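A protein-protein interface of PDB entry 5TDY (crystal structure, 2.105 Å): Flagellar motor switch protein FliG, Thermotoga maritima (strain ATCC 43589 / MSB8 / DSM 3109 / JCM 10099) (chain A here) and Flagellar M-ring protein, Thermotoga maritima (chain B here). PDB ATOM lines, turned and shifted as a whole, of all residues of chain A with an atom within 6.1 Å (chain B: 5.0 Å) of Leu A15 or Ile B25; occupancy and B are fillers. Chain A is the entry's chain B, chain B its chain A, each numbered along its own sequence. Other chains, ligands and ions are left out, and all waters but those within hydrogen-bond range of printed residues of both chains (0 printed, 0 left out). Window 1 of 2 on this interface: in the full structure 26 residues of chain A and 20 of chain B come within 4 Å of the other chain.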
ATOM      1  N   ARG A  10      13.725 -25.909 -17.138  1.00  0.00           N
ATOM      2  CA  ARG A  10      14.792 -26.762 -16.630  1.00  0.00           C
ATOM      3  C   ARG A  10      14.926 -26.656 -15.112  1.00  0.00           C
ATOM      4  O   ARG A  10      15.242 -27.649 -14.439  1.00  0.00           O
ATOM      5  CB  ARG A  10      16.106 -26.405 -17.313  1.00  0.00           C
ATOM      6  CG  ARG A  10      17.266 -27.238 -16.845  1.00  0.00           C
ATOM      7  CD  ARG A  10      18.466 -27.095 -17.751  1.00  0.00           C
ATOM      8  NE  ARG A  10      19.580 -27.907 -17.258  1.00  0.00           N
ATOM      9  CZ  ARG A  10      19.737 -29.198 -17.532  1.00  0.00           C
ATOM     10  NH1 ARG A  10      18.857 -29.822 -18.305  1.00  0.00           N
ATOM     11  NH2 ARG A  10      20.775 -29.860 -17.045  1.00  0.00           N
ATOM     12  N   LYS A  11      14.733 -25.454 -14.556  1.00  0.00           N
ATOM     13  CA  LYS A  11      14.766 -25.314 -13.101  1.00  0.00           C
ATOM     14  C   LYS A  11      13.750 -26.238 -12.442  1.00  0.00           C
ATOM     15  O   LYS A  11      14.077 -26.959 -11.496  1.00  0.00           O
ATOM     16  CB  LYS A  11      14.511 -23.865 -12.691  1.00  0.00           C
ATOM     17  CG  LYS A  11      15.659 -22.923 -13.023  1.00  0.00           C
ATOM     18  CD  LYS A  11      15.571 -21.658 -12.212  1.00  0.00           C
ATOM     19  CE  LYS A  11      15.094 -20.504 -13.044  1.00  0.00           C
ATOM     20  NZ  LYS A  11      15.569 -19.236 -12.435  1.00  0.00           N
ATOM     21  N   ALA A  12      12.512 -26.242 -12.935  1.00  0.00           N
ATOM     22  CA  ALA A  12      11.509 -27.131 -12.351  1.00  0.00           C
ATOM     23  C   ALA A  12      11.915 -28.595 -12.498  1.00  0.00           C
ATOM     24  O   ALA A  12      11.683 -29.402 -11.596  1.00  0.00           O
ATOM     25  CB  ALA A  12      10.139 -26.888 -12.995  1.00  0.00           C
ATOM     26  N   ALA A  13      12.518 -28.959 -13.633  1.00  0.00           N
ATOM     27  CA  ALA A  13      12.921 -30.344 -13.829  1.00  0.00           C
ATOM     28  C   ALA A  13      14.055 -30.725 -12.884  1.00  0.00           C
ATOM     29  O   ALA A  13      14.063 -31.833 -12.333  1.00  0.00           O
ATOM     30  CB  ALA A  13      13.323 -30.578 -15.288  1.00  0.00           C
ATOM     31  N   VAL A  14      15.021 -29.822 -12.687  1.00  0.00           N
ATOM     32  CA  VAL A  14      16.123 -30.098 -11.773  1.00  0.00           C
ATOM     33  C   VAL A  14      15.599 -30.289 -10.354  1.00  0.00           C
ATOM     34  O   VAL A  14      16.040 -31.193  -9.628  1.00  0.00           O
ATOM     35  CB  VAL A  14      17.186 -28.981 -11.857  1.00  0.00           C
ATOM     36  CG1 VAL A  14      18.211 -29.103 -10.710  1.00  0.00           C
ATOM     37  CG2 VAL A  14      17.902 -29.016 -13.226  1.00  0.00           C
ATOM     38  N   LEU A  15      14.619 -29.474  -9.946  1.00  0.00           N
ATOM     39  CA  LEU A  15      14.097 -29.600  -8.590  1.00  0.00           C
ATOM     40  C   LEU A  15      13.423 -30.948  -8.394  1.00  0.00           C
ATOM     41  O   LEU A  15      13.649 -31.624  -7.379  1.00  0.00           O
ATOM     42  CB  LEU A  15      13.120 -28.458  -8.280  1.00  0.00           C
ATOM     43  CG  LEU A  15      12.572 -28.335  -6.850  1.00  0.00           C
ATOM     44  CD1 LEU A  15      13.684 -27.929  -5.903  1.00  0.00           C
ATOM     45  CD2 LEU A  15      11.450 -27.321  -6.798  1.00  0.00           C
ATOM     46  N   LEU A  16      12.601 -31.369  -9.363  1.00  0.00           N
ATOM     47  CA  LEU A  16      11.896 -32.637  -9.195  1.00  0.00           C
ATOM     48  C   LEU A  16      12.856 -33.821  -9.252  1.00  0.00           C
ATOM     49  O   LEU A  16      12.645 -34.822  -8.563  1.00  0.00           O
ATOM     50  CB  LEU A  16      10.788 -32.772 -10.242  1.00  0.00           C
ATOM     51  CG  LEU A  16       9.652 -31.748 -10.061  1.00  0.00           C
ATOM     52  CD1 LEU A  16       8.748 -31.762 -11.269  1.00  0.00           C
ATOM     53  CD2 LEU A  16       8.851 -32.032  -8.771  1.00  0.00           C
ATOM     54  N   VAL A  17      13.899 -33.753 -10.082  1.00  0.00           N
ATOM     55  CA  VAL A  17      14.893 -34.823 -10.068  1.00  0.00           C
ATOM     56  C   VAL A  17      15.573 -34.884  -8.706  1.00  0.00           C
ATOM     57  O   VAL A  17      15.748 -35.963  -8.131  1.00  0.00           O
ATOM     58  CB  VAL A  17      15.901 -34.643 -11.216  1.00  0.00           C
ATOM     59  CG1 VAL A  17      17.166 -35.479 -10.977  1.00  0.00           C
ATOM     60  CG2 VAL A  17      15.260 -35.057 -12.561  1.00  0.00           C
ATOM     61  N   ALA A  18      15.906 -33.721  -8.144  1.00  0.00           N
ATOM     62  CA  ALA A  18      16.565 -33.659  -6.837  1.00  0.00           C
ATOM     63  C   ALA A  18      15.690 -34.211  -5.725  1.00  0.00           C
ATOM     64  O   ALA A  18      16.205 -34.700  -4.711  1.00  0.00           O
ATOM     65  CB  ALA A  18      16.952 -32.210  -6.515  1.00  0.00           C
ATOM     66  N   LEU A  19      14.369 -34.108  -5.871  1.00  0.00           N
ATOM     67  CA  LEU A  19      13.484 -34.653  -4.856  1.00  0.00           C
ATOM     68  C   LEU A  19      13.469 -36.181  -4.874  1.00  0.00           C
ATOM     69  O   LEU A  19      13.174 -36.798  -3.848  1.00  0.00           O
ATOM     70  CB  LEU A  19      12.072 -34.090  -5.052  1.00  0.00           C
ATOM     71  CG  LEU A  19      11.796 -32.728  -4.397  1.00  0.00           C
ATOM     72  CD1 LEU A  19      10.574 -32.058  -5.013  1.00  0.00           C
ATOM     73  CD2 LEU A  19      11.619 -32.867  -2.903  1.00  0.00           C
ATOM     74  N   GLY A  20      13.820 -36.805  -5.996  1.00  0.00           N
ATOM     75  CA  GLY A  20      13.693 -38.240  -6.111  1.00  0.00           C
ATOM     76  C   GLY A  20      12.267 -38.618  -6.459  1.00  0.00           C
ATOM     77  O   GLY A  20      11.335 -37.830  -6.275  1.00  0.00           O
ATOM     78  N   VAL A  27       4.538 -34.317  -5.129  1.00  0.00           N
ATOM     79  CA  VAL A  27       4.421 -32.917  -5.549  1.00  0.00           C
ATOM     80  C   VAL A  27       3.547 -32.799  -6.793  1.00  0.00           C
ATOM     81  O   VAL A  27       2.675 -31.922  -6.882  1.00  0.00           O
ATOM     82  CB  VAL A  27       5.815 -32.305  -5.786  1.00  0.00           C
ATOM     83  CG1 VAL A  27       5.703 -30.954  -6.505  1.00  0.00           C
ATOM     84  CG2 VAL A  27       6.564 -32.149  -4.477  1.00  0.00           C
ATOM     85  N   VAL A  57      19.669 -24.093  -8.419  1.00  0.00           N
ATOM     86  CA  VAL A  57      18.226 -24.299  -8.367  1.00  0.00           C
ATOM     87  C   VAL A  57      17.762 -24.413  -6.922  1.00  0.00           C
ATOM     88  O   VAL A  57      16.767 -23.794  -6.517  1.00  0.00           O
ATOM     89  CB  VAL A  57      17.832 -25.537  -9.196  1.00  0.00           C
ATOM     90  CG1 VAL A  57      16.369 -25.902  -8.955  1.00  0.00           C
ATOM     91  CG2 VAL A  57      18.090 -25.285 -10.672  1.00  0.00           C
ATOM     92  N   LEU A  58      18.501 -25.162  -6.109  1.00  0.00           N
ATOM     93  CA  LEU A  58      18.089 -25.356  -4.724  1.00  0.00           C
ATOM     94  C   LEU A  58      18.116 -24.041  -3.948  1.00  0.00           C
ATOM     95  O   LEU A  58      17.214 -23.767  -3.149  1.00  0.00           O
ATOM     96  CB  LEU A  58      18.980 -26.406  -4.063  1.00  0.00           C
ATOM     97  CG  LEU A  58      18.711 -27.831  -4.560  1.00  0.00           C
ATOM     98  CD1 LEU A  58      19.647 -28.830  -3.882  1.00  0.00           C
ATOM     99  CD2 LEU A  58      17.257 -28.230  -4.338  1.00  0.00           C
ATOM    100  N   PHE A  61      15.122 -21.956  -5.059  1.00  0.00           N
ATOM    101  CA  PHE A  61      13.906 -22.572  -4.535  1.00  0.00           C
ATOM    102  C   PHE A  61      13.675 -22.209  -3.073  1.00  0.00           C
ATOM    103  O   PHE A  61      12.548 -21.886  -2.677  1.00  0.00           O
ATOM    104  CB  PHE A  61      13.952 -24.093  -4.647  1.00  0.00           C
ATOM    105  CG  PHE A  61      12.880 -24.746  -3.824  1.00  0.00           C
ATOM    106  CD1 PHE A  61      11.564 -24.752  -4.271  1.00  0.00           C
ATOM    107  CD2 PHE A  61      13.159 -25.256  -2.569  1.00  0.00           C
ATOM    108  CE1 PHE A  61      10.541 -25.314  -3.484  1.00  0.00           C
ATOM    109  CE2 PHE A  61      12.151 -25.814  -1.781  1.00  0.00           C
ATOM    110  CZ  PHE A  61      10.851 -25.848  -2.241  1.00  0.00           C
ATOM    111  N   LEU B  14      15.271 -28.666   1.757  1.00  0.00           N
ATOM    112  CA  LEU B  14      14.252 -29.084   0.799  1.00  0.00           C
ATOM    113  C   LEU B  14      13.367 -30.170   1.396  1.00  0.00           C
ATOM    114  O   LEU B  14      12.134 -30.099   1.317  1.00  0.00           O
ATOM    115  CB  LEU B  14      14.907 -29.585  -0.491  1.00  0.00           C
ATOM    116  CG  LEU B  14      13.969 -30.227  -1.526  1.00  0.00           C
ATOM    117  CD1 LEU B  14      12.946 -29.205  -1.997  1.00  0.00           C
ATOM    118  CD2 LEU B  14      14.767 -30.770  -2.707  1.00  0.00           C
ATOM    119  N   ILE B  17      10.913 -28.742   3.872  1.00  0.00           N
ATOM    120  CA  ILE B  17       9.836 -28.087   3.206  1.00  0.00           C
ATOM    121  C   ILE B  17       8.801 -29.087   2.692  1.00  0.00           C
ATOM    122  O   ILE B  17       7.648 -28.844   2.799  1.00  0.00           O
ATOM    123  CB  ILE B  17      10.337 -27.122   2.128  1.00  0.00           C
ATOM    124  CG1 ILE B  17      10.976 -25.929   2.806  1.00  0.00           C
ATOM    125  CG2 ILE B  17       9.197 -26.623   1.278  1.00  0.00           C
ATOM    126  CD1 ILE B  17      11.630 -24.957   1.884  1.00  0.00           C
ATOM    127  N   PHE B  18       9.267 -30.194   2.153  1.00  0.00           N
ATOM    128  CA  PHE B  18       8.395 -31.220   1.657  1.00  0.00           C
ATOM    129  C   PHE B  18       7.529 -31.790   2.750  1.00  0.00           C
ATOM    130  O   PHE B  18       6.361 -31.860   2.593  1.00  0.00           O
ATOM    131  CB  PHE B  18       9.126 -32.289   0.860  1.00  0.00           C
ATOM    132  CG  PHE B  18       8.250 -33.429   0.421  1.00  0.00           C
ATOM    133  CD1 PHE B  18       7.654 -33.446  -0.806  1.00  0.00           C
ATOM    134  CD2 PHE B  18       8.007 -34.462   1.251  1.00  0.00           C
ATOM    135  CE1 PHE B  18       6.856 -34.494  -1.191  1.00  0.00           C
ATOM    136  CE2 PHE B  18       7.214 -35.510   0.873  1.00  0.00           C
ATOM    137  CZ  PHE B  18       6.628 -35.514  -0.360  1.00  0.00           C
ATOM    138  N   SER B  21       4.787 -29.038   3.529  1.00  0.00           N
ATOM    139  CA  SER B  21       3.775 -28.796   2.506  1.00  0.00           C
ATOM    140  C   SER B  21       4.306 -29.082   1.103  1.00  0.00           C
ATOM    141  O   SER B  21       5.024 -28.255   0.526  1.00  0.00           O
ATOM    142  CB  SER B  21       3.282 -27.352   2.582  1.00  0.00           C
ATOM    143  OG  SER B  21       2.738 -26.953   1.335  1.00  0.00           O
ATOM    144  N   PRO B  22       3.974 -30.234   0.519  1.00  0.00           N
ATOM    145  CA  PRO B  22       4.275 -30.435  -0.907  1.00  0.00           C
ATOM    146  C   PRO B  22       3.611 -29.416  -1.820  1.00  0.00           C
ATOM    147  O   PRO B  22       4.117 -29.172  -2.924  1.00  0.00           O
ATOM    148  CB  PRO B  22       3.750 -31.858  -1.180  1.00  0.00           C
ATOM    149  CG  PRO B  22       3.738 -32.531   0.146  1.00  0.00           C
ATOM    150  CD  PRO B  22       3.393 -31.437   1.139  1.00  0.00           C
ATOM    151  N   SER B  23       2.485 -28.817  -1.415  1.00  0.00           N
ATOM    152  CA  SER B  23       1.827 -27.869  -2.313  1.00  0.00           C
ATOM    153  C   SER B  23       2.622 -26.573  -2.456  1.00  0.00           C
ATOM    154  O   SER B  23       2.530 -25.911  -3.496  1.00  0.00           O
ATOM    155  CB  SER B  23       0.396 -27.574  -1.848  1.00  0.00           C
ATOM    156  OG  SER B  23       0.371 -26.885  -0.614  1.00  0.00           O
ATOM    157  N   ASP B  24       3.417 -26.202  -1.446  1.00  0.00           N
ATOM    158  CA  ASP B  24       4.299 -25.046  -1.602  1.00  0.00           C
ATOM    159  C   ASP B  24       5.388 -25.300  -2.634  1.00  0.00           C
ATOM    160  O   ASP B  24       5.825 -24.368  -3.325  1.00  0.00           O
ATOM    161  CB  ASP B  24       4.948 -24.683  -0.268  1.00  0.00           C
ATOM    162  CG  ASP B  24       3.965 -24.065   0.701  1.00  0.00           C
ATOM    163  OD1 ASP B  24       2.982 -23.453   0.229  1.00  0.00           O
ATOM    164  OD2 ASP B  24       4.165 -24.207   1.925  1.00  0.00           O
ATOM    165  N   ILE B  25       5.863 -26.542  -2.729  1.00  0.00           N
ATOM    166  CA  ILE B  25       6.812 -26.884  -3.780  1.00  0.00           C
ATOM    167  C   ILE B  25       6.141 -26.820  -5.150  1.00  0.00           C
ATOM    168  O   ILE B  25       6.701 -26.265  -6.102  1.00  0.00           O
ATOM    169  CB  ILE B  25       7.424 -28.267  -3.520  1.00  0.00           C
ATOM    170  CG1 ILE B  25       8.083 -28.284  -2.140  1.00  0.00           C
ATOM    171  CG2 ILE B  25       8.421 -28.595  -4.638  1.00  0.00           C
ATOM    172  CD1 ILE B  25       8.698 -29.635  -1.774  1.00  0.00           C
ATOM    173  N   ALA B  26       4.939 -27.406  -5.271  1.00  0.00           N
ATOM    174  CA  ALA B  26       4.206 -27.356  -6.536  1.00  0.00           C
ATOM    175  C   ALA B  26       4.010 -25.927  -7.021  1.00  0.00           C
ATOM    176  O   ALA B  26       4.079 -25.662  -8.225  1.00  0.00           O
ATOM    177  CB  ALA B  26       2.847 -28.031  -6.399  1.00  0.00           C
ATOM    178  N   GLU B  27       3.724 -25.004  -6.106  1.00  0.00           N
ATOM    179  CA  GLU B  27       3.517 -23.608  -6.489  1.00  0.00           C
ATOM    180  C   GLU B  27       4.759 -23.017  -7.156  1.00  0.00           C
ATOM    181  O   GLU B  27       4.652 -22.310  -8.163  1.00  0.00           O
ATOM    182  CB  GLU B  27       3.123 -22.789  -5.259  1.00  0.00           C
ATOM    183  CG  GLU B  27       2.171 -21.649  -5.572  1.00  0.00           C
ATOM    184  CD  GLU B  27       2.156 -20.585  -4.495  1.00  0.00           C
ATOM    185  OE1 GLU B  27       2.583 -20.874  -3.350  1.00  0.00           O
ATOM    186  OE2 GLU B  27       1.726 -19.456  -4.806  1.00  0.00           O
ATOM    187  N   ILE B  28       5.946 -23.306  -6.615  1.00  0.00           N
ATOM    188  CA  ILE B  28       7.187 -22.809  -7.202  1.00  0.00           C
ATOM    189  C   ILE B  28       7.497 -23.529  -8.515  1.00  0.00           C
ATOM    190  O   ILE B  28       7.987 -22.914  -9.464  1.00  0.00           O
ATOM    191  CB  ILE B  28       8.342 -22.939  -6.192  1.00  0.00           C
ATOM    192  CG1 ILE B  28       8.101 -22.012  -4.999  1.00  0.00           C
ATOM    193  CG2 ILE B  28       9.683 -22.629  -6.866  1.00  0.00           C
ATOM    194  CD1 ILE B  28       9.056 -22.227  -3.860  1.00  0.00           C
ATOM    195  N   VAL B  29       7.201 -24.830  -8.599  1.00  0.00           N
ATOM    196  CA  VAL B  29       7.294 -25.540  -9.880  1.00  0.00           C
ATOM    197  C   VAL B  29       6.446 -24.838 -10.942  1.00  0.00           C
ATOM    198  O   VAL B  29       6.898 -24.606 -12.071  1.00  0.00           O
ATOM    199  CB  VAL B  29       6.864 -27.011  -9.714  1.00  0.00           C
ATOM    200  CG1 VAL B  29       6.624 -27.654 -11.093  1.00  0.00           C
ATOM    201  CG2 VAL B  29       7.899 -27.791  -8.934  1.00  0.00           C
ATOM    202  N   TRP B  32       7.965 -21.448 -12.025  1.00  0.00           N
ATOM    203  CA  TRP B  32       9.137 -21.633 -12.874  1.00  0.00           C
ATOM    204  C   TRP B  32       8.766 -22.109 -14.277  1.00  0.00           C
ATOM    205  O   TRP B  32       9.286 -21.590 -15.276  1.00  0.00           O
ATOM    206  CB  TRP B  32      10.097 -22.619 -12.218  1.00  0.00           C
ATOM    207  CG  TRP B  32      11.053 -21.975 -11.246  1.00  0.00           C
ATOM    208  CD1 TRP B  32      11.283 -20.633 -11.080  1.00  0.00           C
ATOM    209  CD2 TRP B  32      11.899 -22.649 -10.310  1.00  0.00           C
ATOM    210  NE1 TRP B  32      12.231 -20.434 -10.094  1.00  0.00           N
ATOM    211  CE2 TRP B  32      12.627 -21.657  -9.609  1.00  0.00           C
ATOM    212  CE3 TRP B  32      12.113 -23.992  -9.992  1.00  0.00           C
ATOM    213  CZ2 TRP B  32      13.557 -21.972  -8.623  1.00  0.00           C
ATOM    214  CZ3 TRP B  32      13.036 -24.303  -9.006  1.00  0.00           C
ATOM    215  CH2 TRP B  32      13.747 -23.301  -8.337  1.00  0.00           C
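Hydrophobic or aromatic side chains of chain A within 4 Å of the printed part of chain B: Leu A15, Leu A19, Val A27, Val A57, Leu A58 and Phe A61.
Hydrophobic or aromatic side chains of chain B within 4 Å of the printed part of chain A: Leu B14, Ile B17, Ile B25, Ala B26, Ile B28 and Trp B32.
Along chain B the printed residues that touch a printed residue of chain A span positions 14 to 32.
Among the printed residues, 12 pairs touch across the chains.
CB of Lys A11 touches CE3 of Trp B32, at 3.6 Å.
Trp B32 touches Ala A12.
Leu B14 touches Leu A19 (CD2 to CD2, 3.8 Å).
Val A27 touches Ala B26.
Trp B32 touches Val A57.
Leu A58 touches Leu B14.
Leu B14 touches Phe A61.
Phe A61 touches Ile B17 (CE2 to CD1, 3.8 Å).
Ile B28 touches Phe A61.
Phe A61 touches Trp B32.
Leu A15 touches just one residue of chain B: Ile B25.
Printed residues of chain A within 4 Å of Ile B25: Leu A15 and Phe A61.
Of the printed residues of chain A, Ile B17 touches Phe A61 (3.8 Å).
Of the printed residues of chain B, Phe A61 touches Leu B14 (3.5 Å), Ile B17 (3.8 Å), Ile B25 (3.7 Å), Ile B28 (3.4 Å) and Trp B32 (3.8 Å).
Printed residues of chain B within 4 Å of Lys A11: Trp B32.
The nearest printed residue of chain B that does not touch Val A57 is Ile B28 (7.2 Å).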
